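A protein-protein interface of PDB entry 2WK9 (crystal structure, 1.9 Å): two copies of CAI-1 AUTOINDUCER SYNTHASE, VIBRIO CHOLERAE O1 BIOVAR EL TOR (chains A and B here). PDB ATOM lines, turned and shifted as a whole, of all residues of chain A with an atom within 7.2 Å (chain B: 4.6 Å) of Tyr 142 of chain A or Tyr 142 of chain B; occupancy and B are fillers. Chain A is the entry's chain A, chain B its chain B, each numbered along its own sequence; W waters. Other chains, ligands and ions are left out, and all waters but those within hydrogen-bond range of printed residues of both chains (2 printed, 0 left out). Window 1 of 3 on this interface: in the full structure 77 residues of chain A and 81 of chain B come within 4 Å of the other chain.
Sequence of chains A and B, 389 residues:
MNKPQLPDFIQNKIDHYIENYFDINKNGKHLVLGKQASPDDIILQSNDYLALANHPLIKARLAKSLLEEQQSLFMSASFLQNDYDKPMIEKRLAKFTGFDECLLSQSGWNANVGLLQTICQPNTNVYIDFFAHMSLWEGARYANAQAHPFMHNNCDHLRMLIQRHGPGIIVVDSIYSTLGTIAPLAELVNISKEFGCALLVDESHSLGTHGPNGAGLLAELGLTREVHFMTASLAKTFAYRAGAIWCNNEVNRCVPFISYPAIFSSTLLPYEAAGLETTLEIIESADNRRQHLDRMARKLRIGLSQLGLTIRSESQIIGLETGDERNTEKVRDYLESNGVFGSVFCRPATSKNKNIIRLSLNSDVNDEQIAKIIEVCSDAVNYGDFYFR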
ATOM      1  N   TRP A 109     -23.802   8.383  -1.190  1.00  0.00           N
ATOM      2  CA  TRP A 109     -23.241   7.841   0.041  1.00  0.00           C
ATOM      3  C   TRP A 109     -23.226   6.314  -0.018  1.00  0.00           C
ATOM      4  O   TRP A 109     -22.203   5.681   0.226  1.00  0.00           O
ATOM      5  CB  TRP A 109     -24.066   8.302   1.250  1.00  0.00           C
ATOM      6  CG  TRP A 109     -23.582   7.718   2.537  1.00  0.00           C
ATOM      7  CD1 TRP A 109     -23.841   6.463   3.021  1.00  0.00           C
ATOM      8  CD2 TRP A 109     -22.752   8.358   3.507  1.00  0.00           C
ATOM      9  NE1 TRP A 109     -23.214   6.287   4.228  1.00  0.00           N
ATOM     10  CE2 TRP A 109     -22.546   7.437   4.555  1.00  0.00           C
ATOM     11  CE3 TRP A 109     -22.171   9.627   3.597  1.00  0.00           C
ATOM     12  CZ2 TRP A 109     -21.775   7.740   5.675  1.00  0.00           C
ATOM     13  CZ3 TRP A 109     -21.401   9.927   4.710  1.00  0.00           C
ATOM     14  CH2 TRP A 109     -21.210   8.987   5.733  1.00  0.00           C
ATOM     15  N   VAL A 113     -20.084   3.597   0.059  1.00  0.00           N
ATOM     16  CA  VAL A 113     -20.023   2.606   1.134  1.00  0.00           C
ATOM     17  C   VAL A 113     -20.107   1.189   0.572  1.00  0.00           C
ATOM     18  O   VAL A 113     -19.345   0.302   0.969  1.00  0.00           O
ATOM     19  CB  VAL A 113     -21.149   2.826   2.174  1.00  0.00           C
ATOM     20  CG1 VAL A 113     -21.265   1.633   3.094  1.00  0.00           C
ATOM     21  CG2 VAL A 113     -20.882   4.107   2.967  1.00  0.00           C
ATOM     22  N   GLN A 117     -17.161  -1.721   0.626  1.00  0.00           N
ATOM     23  CA  GLN A 117     -17.424  -2.948   1.374  1.00  0.00           C
ATOM     24  C   GLN A 117     -17.128  -4.153   0.490  1.00  0.00           C
ATOM     25  O   GLN A 117     -16.627  -5.177   0.956  1.00  0.00           O
ATOM     26  CB  GLN A 117     -18.882  -2.994   1.868  1.00  0.00           C
ATOM     27  CG  GLN A 117     -19.231  -4.278   2.627  1.00  0.00           C
ATOM     28  CD  GLN A 117     -20.653  -4.303   3.184  1.00  0.00           C
ATOM     29  OE1 GLN A 117     -21.434  -3.364   3.002  1.00  0.00           O
ATOM     30  NE2 GLN A 117     -20.990  -5.390   3.866  1.00  0.00           N
ATOM     31  N   MET A 134     -16.631  12.345   3.051  1.00  0.00           N
ATOM     32  CA  MET A 134     -16.843  11.549   4.263  1.00  0.00           C
ATOM     33  C   MET A 134     -17.357  10.132   3.988  1.00  0.00           C
ATOM     34  O   MET A 134     -17.009   9.202   4.704  1.00  0.00           O
ATOM     35  CB  MET A 134     -17.797  12.268   5.218  1.00  0.00           C
ATOM     36  CG  MET A 134     -18.038  11.520   6.525  1.00  0.00           C
ATOM     37  SD  MET A 134     -16.567  11.468   7.565  1.00  0.00           S
ATOM     38  CE  MET A 134     -16.633  13.104   8.293  1.00  0.00           C
ATOM     39  N   SER A 135     -18.183   9.971   2.955  1.00  0.00           N
ATOM     40  CA  SER A 135     -18.713   8.655   2.601  1.00  0.00           C
ATOM     41  C   SER A 135     -17.604   7.668   2.238  1.00  0.00           C
ATOM     42  O   SER A 135     -17.739   6.466   2.464  1.00  0.00           O
ATOM     43  CB  SER A 135     -19.741   8.759   1.457  1.00  0.00           C
ATOM     44  OG  SER A 135     -19.158   9.344   0.287  1.00  0.00           O
ATOM     45  N   LEU A 136     -16.510   8.179   1.676  1.00  0.00           N
ATOM     46  CA  LEU A 136     -15.374   7.336   1.312  1.00  0.00           C
ATOM     47  C   LEU A 136     -14.563   6.963   2.548  1.00  0.00           C
ATOM     48  O   LEU A 136     -14.140   5.819   2.709  1.00  0.00           O
ATOM     49  CB  LEU A 136     -14.484   8.037   0.283  1.00  0.00           C
ATOM     50  CG  LEU A 136     -15.146   8.269  -1.074  1.00  0.00           C
ATOM     51  CD1 LEU A 136     -14.417   9.364  -1.826  1.00  0.00           C
ATOM     52  CD2 LEU A 136     -15.185   6.963  -1.879  1.00  0.00           C
ATOM     53  N   TRP A 137     -14.354   7.936   3.425  1.00  0.00           N
ATOM     54  CA  TRP A 137     -13.691   7.673   4.695  1.00  0.00           C
ATOM     55  C   TRP A 137     -14.466   6.632   5.493  1.00  0.00           C
ATOM     56  O   TRP A 137     -13.898   5.651   5.985  1.00  0.00           O
ATOM     57  CB  TRP A 137     -13.570   8.969   5.491  1.00  0.00           C
ATOM     58  CG  TRP A 137     -12.434   9.825   5.033  1.00  0.00           C
ATOM     59  CD1 TRP A 137     -12.483  10.855   4.138  1.00  0.00           C
ATOM     60  CD2 TRP A 137     -11.071   9.714   5.445  1.00  0.00           C
ATOM     61  NE1 TRP A 137     -11.228  11.396   3.972  1.00  0.00           N
ATOM     62  CE2 TRP A 137     -10.344  10.713   4.765  1.00  0.00           C
ATOM     63  CE3 TRP A 137     -10.393   8.865   6.323  1.00  0.00           C
ATOM     64  CZ2 TRP A 137      -8.977  10.888   4.940  1.00  0.00           C
ATOM     65  CZ3 TRP A 137      -9.033   9.040   6.495  1.00  0.00           C
ATOM     66  CH2 TRP A 137      -8.341  10.043   5.806  1.00  0.00           C
ATOM     67  N   GLU A 138     -15.772   6.849   5.614  1.00  0.00           N
ATOM     68  CA  GLU A 138     -16.618   5.935   6.371  1.00  0.00           C
ATOM     69  C   GLU A 138     -16.717   4.573   5.698  1.00  0.00           C
ATOM     70  O   GLU A 138     -16.677   3.543   6.364  1.00  0.00           O
ATOM     71  CB  GLU A 138     -17.999   6.544   6.599  1.00  0.00           C
ATOM     72  CG  GLU A 138     -17.964   7.710   7.570  1.00  0.00           C
ATOM     73  CD  GLU A 138     -17.654   7.270   8.993  1.00  0.00           C
ATOM     74  OE1 GLU A 138     -18.601   6.912   9.721  1.00  0.00           O
ATOM     75  OE2 GLU A 138     -16.467   7.289   9.383  1.00  0.00           O
ATOM     76  N   GLY A 139     -16.838   4.567   4.377  1.00  0.00           N
ATOM     77  CA  GLY A 139     -16.859   3.320   3.633  1.00  0.00           C
ATOM     78  C   GLY A 139     -15.692   2.422   3.992  1.00  0.00           C
ATOM     79  O   GLY A 139     -15.857   1.224   4.245  1.00  0.00           O
ATOM     80  N   ALA A 140     -14.499   3.010   4.018  1.00  0.00           N
ATOM     81  CA  ALA A 140     -13.295   2.263   4.336  1.00  0.00           C
ATOM     82  C   ALA A 140     -13.332   1.808   5.788  1.00  0.00           C
ATOM     83  O   ALA A 140     -12.964   0.683   6.107  1.00  0.00           O
ATOM     84  CB  ALA A 140     -12.065   3.120   4.078  1.00  0.00           C
ATOM     85  N   ARG A 141     -13.793   2.695   6.661  1.00  0.00           N
ATOM     86  CA  ARG A 141     -13.836   2.417   8.089  1.00  0.00           C
ATOM     87  C   ARG A 141     -14.806   1.278   8.417  1.00  0.00           C
ATOM     88  O   ARG A 141     -14.494   0.400   9.223  1.00  0.00           O
ATOM     89  CB  ARG A 141     -14.205   3.691   8.854  1.00  0.00           C
ATOM     90  CG  ARG A 141     -14.175   3.544  10.369  1.00  0.00           C
ATOM     91  CD  ARG A 141     -15.055   4.596  11.016  1.00  0.00           C
ATOM     92  NE  ARG A 141     -15.618   4.092  12.263  1.00  0.00           N
ATOM     93  CZ  ARG A 141     -16.826   4.394  12.720  1.00  0.00           C
ATOM     94  NH1 ARG A 141     -17.631   5.200  12.035  1.00  0.00           N
ATOM     95  NH2 ARG A 141     -17.233   3.873  13.864  1.00  0.00           N
ATOM     96  N   TYR A 142     -15.980   1.291   7.789  1.00  0.00           N
ATOM     97  CA  TYR A 142     -16.963   0.232   7.993  1.00  0.00           C
ATOM     98  C   TYR A 142     -16.403  -1.102   7.534  1.00  0.00           C
ATOM     99  O   TYR A 142     -16.774  -2.157   8.061  1.00  0.00           O
ATOM    100  CB  TYR A 142     -18.263   0.513   7.232  1.00  0.00           C
ATOM    101  CG  TYR A 142     -18.949   1.815   7.581  1.00  0.00           C
ATOM    102  CD1 TYR A 142     -18.681   2.475   8.777  1.00  0.00           C
ATOM    103  CD2 TYR A 142     -19.890   2.370   6.723  1.00  0.00           C
ATOM    104  CE1 TYR A 142     -19.318   3.672   9.095  1.00  0.00           C
ATOM    105  CE2 TYR A 142     -20.535   3.554   7.035  1.00  0.00           C
ATOM    106  CZ  TYR A 142     -20.245   4.203   8.218  1.00  0.00           C
ATOM    107  OH  TYR A 142     -20.882   5.387   8.507  1.00  0.00           O
ATOM    108  N   ALA A 143     -15.522  -1.048   6.539  1.00  0.00           N
ATOM    109  CA  ALA A 143     -14.912  -2.244   5.975  1.00  0.00           C
ATOM    110  C   ALA A 143     -13.695  -2.678   6.785  1.00  0.00           C
ATOM    111  O   ALA A 143     -13.058  -3.680   6.463  1.00  0.00           O
ATOM    112  CB  ALA A 143     -14.518  -2.000   4.519  1.00  0.00           C
ATOM    113  N   ASN A 144     -13.374  -1.914   7.827  1.00  0.00           N
ATOM    114  CA  ASN A 144     -12.223  -2.206   8.677  1.00  0.00           C
ATOM    115  C   ASN A 144     -10.903  -2.189   7.909  1.00  0.00           C
ATOM    116  O   ASN A 144      -9.959  -2.898   8.256  1.00  0.00           O
ATOM    117  CB  ASN A 144     -12.411  -3.542   9.401  1.00  0.00           C
ATOM    118  CG  ASN A 144     -13.477  -3.469  10.473  1.00  0.00           C
ATOM    119  OD1 ASN A 144     -14.511  -4.130  10.384  1.00  0.00           O
ATOM    120  ND2 ASN A 144     -13.242  -2.641  11.486  1.00  0.00           N
ATOM    121  N   ALA A 145     -10.844  -1.363   6.869  1.00  0.00           N
ATOM    122  CA  ALA A 145      -9.658  -1.267   6.030  1.00  0.00           C
ATOM    123  C   ALA A 145      -8.575  -0.461   6.730  1.00  0.00           C
ATOM    124  O   ALA A 145      -8.839   0.241   7.707  1.00  0.00           O
ATOM    125  CB  ALA A 145     -10.008  -0.628   4.694  1.00  0.00           C
ATOM    126  N   TYR A 260     -24.159  -3.833   2.325  1.00  0.00           N
ATOM    127  CA  TYR A 260     -25.273  -3.825   3.267  1.00  0.00           C
ATOM    128  C   TYR A 260     -26.390  -2.852   2.878  1.00  0.00           C
ATOM    129  O   TYR A 260     -27.563  -3.227   2.886  1.00  0.00           O
ATOM    130  CB  TYR A 260     -24.792  -3.564   4.692  1.00  0.00           C
ATOM    131  CG  TYR A 260     -24.174  -4.780   5.349  1.00  0.00           C
ATOM    132  CD1 TYR A 260     -24.171  -6.013   4.708  1.00  0.00           C
ATOM    133  CD2 TYR A 260     -23.622  -4.697   6.620  1.00  0.00           C
ATOM    134  CE1 TYR A 260     -23.621  -7.133   5.316  1.00  0.00           C
ATOM    135  CE2 TYR A 260     -23.072  -5.808   7.237  1.00  0.00           C
ATOM    136  CZ  TYR A 260     -23.078  -7.022   6.582  1.00  0.00           C
ATOM    137  OH  TYR A 260     -22.534  -8.128   7.197  1.00  0.00           O
ATOM    138  N   PRO A 261     -26.036  -1.599   2.540  1.00  0.00           N
ATOM    139  CA  PRO A 261     -27.076  -0.676   2.067  1.00  0.00           C
ATOM    140  C   PRO A 261     -27.801  -1.225   0.849  1.00  0.00           C
ATOM    141  O   PRO A 261     -29.002  -1.001   0.712  1.00  0.00           O
ATOM    142  CB  PRO A 261     -26.285   0.574   1.688  1.00  0.00           C
ATOM    143  CG  PRO A 261     -25.094   0.533   2.587  1.00  0.00           C
ATOM    144  CD  PRO A 261     -24.733  -0.928   2.688  1.00  0.00           C
ATOM    145  N   TRP B 109     -33.220   2.480   6.877  1.00  0.00           N
ATOM    146  CA  TRP B 109     -31.830   2.206   7.224  1.00  0.00           C
ATOM    147  C   TRP B 109     -31.182   3.451   7.835  1.00  0.00           C
ATOM    148  O   TRP B 109     -30.530   3.372   8.886  1.00  0.00           O
ATOM    149  CB  TRP B 109     -31.033   1.733   5.996  1.00  0.00           C
ATOM    150  CG  TRP B 109     -29.555   1.591   6.240  1.00  0.00           C
ATOM    151  CD1 TRP B 109     -28.622   2.602   6.286  1.00  0.00           C
ATOM    152  CD2 TRP B 109     -28.832   0.372   6.467  1.00  0.00           C
ATOM    153  NE1 TRP B 109     -27.376   2.084   6.533  1.00  0.00           N
ATOM    154  CE2 TRP B 109     -27.473   0.722   6.647  1.00  0.00           C
ATOM    155  CE3 TRP B 109     -29.198  -0.976   6.531  1.00  0.00           C
ATOM    156  CZ2 TRP B 109     -26.485  -0.230   6.892  1.00  0.00           C
ATOM    157  CZ3 TRP B 109     -28.212  -1.919   6.775  1.00  0.00           C
ATOM    158  CH2 TRP B 109     -26.873  -1.542   6.954  1.00  0.00           C
ATOM    159  N   VAL B 113     -29.644   4.106  11.650  1.00  0.00           N
ATOM    160  CA  VAL B 113     -28.230   4.430  11.752  1.00  0.00           C
ATOM    161  C   VAL B 113     -28.026   5.827  12.340  1.00  0.00           C
ATOM    162  O   VAL B 113     -27.139   6.035  13.175  1.00  0.00           O
ATOM    163  CB  VAL B 113     -27.538   4.329  10.379  1.00  0.00           C
ATOM    164  CG1 VAL B 113     -26.253   5.126  10.378  1.00  0.00           C
ATOM    165  CG2 VAL B 113     -27.274   2.862  10.035  1.00  0.00           C
ATOM    166  N   GLU B 138     -25.668  -2.470  12.519  1.00  0.00           N
ATOM    167  CA  GLU B 138     -24.661  -1.596  11.919  1.00  0.00           C
ATOM    168  C   GLU B 138     -24.657  -0.204  12.551  1.00  0.00           C
ATOM    169  O   GLU B 138     -23.595   0.384  12.765  1.00  0.00           O
ATOM    170  CB  GLU B 138     -24.854  -1.502  10.399  1.00  0.00           C
ATOM    171  CG  GLU B 138     -24.468  -2.769   9.648  1.00  0.00           C
ATOM    172  CD  GLU B 138     -22.993  -3.114   9.809  1.00  0.00           C
ATOM    173  OE1 GLU B 138     -22.205  -2.790   8.897  1.00  0.00           O
ATOM    174  OE2 GLU B 138     -22.618  -3.697  10.851  1.00  0.00           O
ATOM    175  N   GLY B 139     -25.841   0.330  12.838  1.00  0.00           N
ATOM    176  CA  GLY B 139     -25.930   1.631  13.475  1.00  0.00           C
ATOM    177  C   GLY B 139     -25.128   1.659  14.766  1.00  0.00           C
ATOM    178  O   GLY B 139     -24.387   2.613  15.031  1.00  0.00           O
ATOM    179  N   ALA B 140     -25.268   0.605  15.567  1.00  0.00           N
ATOM    180  CA  ALA B 140     -24.540   0.501  16.830  1.00  0.00           C
ATOM    181  C   ALA B 140     -23.046   0.370  16.576  1.00  0.00           C
ATOM    182  O   ALA B 140     -22.236   0.993  17.253  1.00  0.00           O
ATOM    183  CB  ALA B 140     -25.039  -0.694  17.642  1.00  0.00           C
ATOM    184  N   ARG B 141     -22.693  -0.444  15.590  1.00  0.00           N
ATOM    185  CA  ARG B 141     -21.296  -0.680  15.248  1.00  0.00           C
ATOM    186  C   ARG B 141     -20.598   0.582  14.718  1.00  0.00           C
ATOM    187  O   ARG B 141     -19.443   0.840  15.055  1.00  0.00           O
ATOM    188  CB  ARG B 141     -21.200  -1.828  14.245  1.00  0.00           C
ATOM    189  CG  ARG B 141     -19.789  -2.240  13.891  1.00  0.00           C
ATOM    190  CD  ARG B 141     -19.798  -3.232  12.749  1.00  0.00           C
ATOM    191  NE  ARG B 141     -18.505  -3.263  12.085  1.00  0.00           N
ATOM    192  CZ  ARG B 141     -18.288  -2.901  10.826  1.00  0.00           C
ATOM    193  NH1 ARG B 141     -19.289  -2.512  10.041  1.00  0.00           N
ATOM    194  NH2 ARG B 141     -17.064  -2.976  10.343  1.00  0.00           N
ATOM    195  N   TYR B 142     -21.290   1.375  13.903  1.00  0.00           N
ATOM    196  CA  TYR B 142     -20.690   2.612  13.391  1.00  0.00           C
ATOM    197  C   TYR B 142     -20.408   3.579  14.527  1.00  0.00           C
ATOM    198  O   TYR B 142     -19.475   4.376  14.461  1.00  0.00           O
ATOM    199  CB  TYR B 142     -21.598   3.326  12.389  1.00  0.00           C
ATOM    200  CG  TYR B 142     -21.941   2.543  11.154  1.00  0.00           C
ATOM    201  CD1 TYR B 142     -21.221   1.413  10.795  1.00  0.00           C
ATOM    202  CD2 TYR B 142     -22.976   2.952  10.331  1.00  0.00           C
ATOM    203  CE1 TYR B 142     -21.545   0.701   9.657  1.00  0.00           C
ATOM    204  CE2 TYR B 142     -23.299   2.257   9.197  1.00  0.00           C
ATOM    205  CZ  TYR B 142     -22.583   1.133   8.867  1.00  0.00           C
ATOM    206  OH  TYR B 142     -22.916   0.443   7.733  1.00  0.00           O
ATOM    207  N   ALA B 143     -21.243   3.523  15.555  1.00  0.00           N
ATOM    208  CA  ALA B 143     -21.108   4.415  16.696  1.00  0.00           C
ATOM    209  C   ALA B 143     -20.099   3.867  17.694  1.00  0.00           C
ATOM    210  O   ALA B 143     -19.869   4.465  18.747  1.00  0.00           O
ATOM    211  CB  ALA B 143     -22.455   4.628  17.359  1.00  0.00           C
ATOM    212  N   ASN B 144     -19.500   2.728  17.352  1.00  0.00           N
ATOM    213  CA  ASN B 144     -18.562   2.046  18.238  1.00  0.00           C
ATOM    214  C   ASN B 144     -19.169   1.722  19.605  1.00  0.00           C
ATOM    215  O   ASN B 144     -18.474   1.726  20.626  1.00  0.00           O
ATOM    216  CB  ASN B 144     -17.280   2.860  18.398  1.00  0.00           C
ATOM    217  CG  ASN B 144     -16.444   2.865  17.136  1.00  0.00           C
ATOM    218  OD1 ASN B 144     -16.302   3.895  16.486  1.00  0.00           O
ATOM    219  ND2 ASN B 144     -15.912   1.702  16.769  1.00  0.00           N
HETATM  220  O   HOH W   1     -16.770  -5.183   7.928  1.00  0.00           O
HETATM  221  O   HOH W   2     -14.751   1.571  13.690  1.00  0.00           O
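Among the printed residues, pairs that only touch across the chains: Tyr 260 of chain A with Glu 138 of chain B, Tyr 142 of chain A with Tyr 142 of chain B, Tyr 260 of chain A with Trp 109 of chain B and Arg 141 of chain A with Arg 141 of chain B.
Of chain B, only Arg 141 (2.4 Å) and Tyr 142 (3.4 Å) come within 4 Å of Tyr 142 of chain A. Of the printed residues of chain B, Asn 144 of chain A touches Arg 141 (2.8 Å). Ala 145 of chain A touches none of the printed residues of chain B. Of the printed residues of chain A, Trp 109 of chain B touches Tyr 260. Printed residues of chain A within 4 Å of Glu 138 of chain B: Tyr 260. Ala 140 of chain B touches none of the printed residues of chain A. Of the printed residues of chain A, Arg 141 of chain B touches Arg 141, Tyr 142 and Asn 144. Tyr 142 of chain B touches just these residues of chain A: Arg 141 (2.4 Å) and Tyr 142 (3.4 Å). Of the printed residues of chain A, Asn 144 of chain B touches Arg 141 (2.8 Å). The nearest printed residue of chain B that does not touch Tyr 142 of chain A is Glu 138 of chain B (5.4 Å). The nearest residue of chain A that does not touch Tyr 142 of chain B is Val 113 of chain A (5.1 Å). The nearest printed residue of chain A that does not touch Asn 144 of chain B is Asn 144 of chain A (7.3 Å).
Of the 17 printed residues of chain A, 4 touch a printed residue of chain B. Hydrophobic or aromatic side chains of chain A that line the printed part of chain B: Tyr 142 and Tyr 260. Among the printed residues, no Asp or Glu carboxylate lies within 4 Å of a Lys or Arg side-chain nitrogen of the other chain.
Arg 141 of chain B touches its own counterpart, Arg 141 of chain A. Arg 141 of chain A touches Tyr 142 of chain B, and with the chains exchanged Tyr 142 of chain A touches Arg 141 of chain B. Arg 141 of chain A touches Asn 144 of chain B, and with the chains exchanged Asn 144 of chain A touches Arg 141 of chain B. Tyr 142 of chain A touches its own counterpart, Tyr 142 of chain B. Positions printed for both chains: 109, 113, 138, 139, 140, 141, 142, 143 and 144. Of the 8 pairs that touch across the chains among the printed residues, 6 have their exchanged pair printed and touching as well.
The side-chain carboxylate of Glu 138 of chain B is in salt-bridge range of the guanidinium group of Arg 141 of chain B (3.1 Å). The side-chain amide oxygen of Gln 117 of chain A is in hydrogen-bond range of the backbone NH of Tyr 260 of chain A (2.8 Å). The side-chain carboxylate (OE1) of Glu 138 of chain A is in hydrogen-bond range of the side-chain hydroxyl (OH) of Tyr 142 of chain A (3.0 Å). NH1 of Arg 141 of chain A is in salt-bridge range of OE1 of Glu 138 of chain A (3.0 Å).
The guanidinium group (NH2) of Arg 141 of chain A sits at hydrogen-bond distance from the side-chain amide oxygen (OD1) of Asn 144 of chain B, at 2.8 Å. The side-chain amide oxygen (OD1) of Asn 144 of chain A sits at hydrogen-bond distance from the guanidinium group (NH2) of Arg 141 of chain B. The backbone carbonyl oxygen of Tyr 142 of chain B is in hydrogen-bond range of the guanidinium group of Arg 141 of chain A. NH2 of Arg 141 of chain B is in hydrogen-bond range of O of Tyr 142 of chain A (2.4 Å).
Water W2 bridges the guanidinium group (NE) of Arg 141 of chain A (3.0 Å) and the side-chain amide nitrogen (ND2) of Asn 144 of chain B (3.3 Å). Water W1 lies within hydrogen-bond range of the backbone carbonyl oxygen (O) of Tyr 142 of chain A, the guanidinium group (NH2) of Arg 141 of chain B and the side-chain amide oxygen (OD1) of Asn 144 of chain A.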
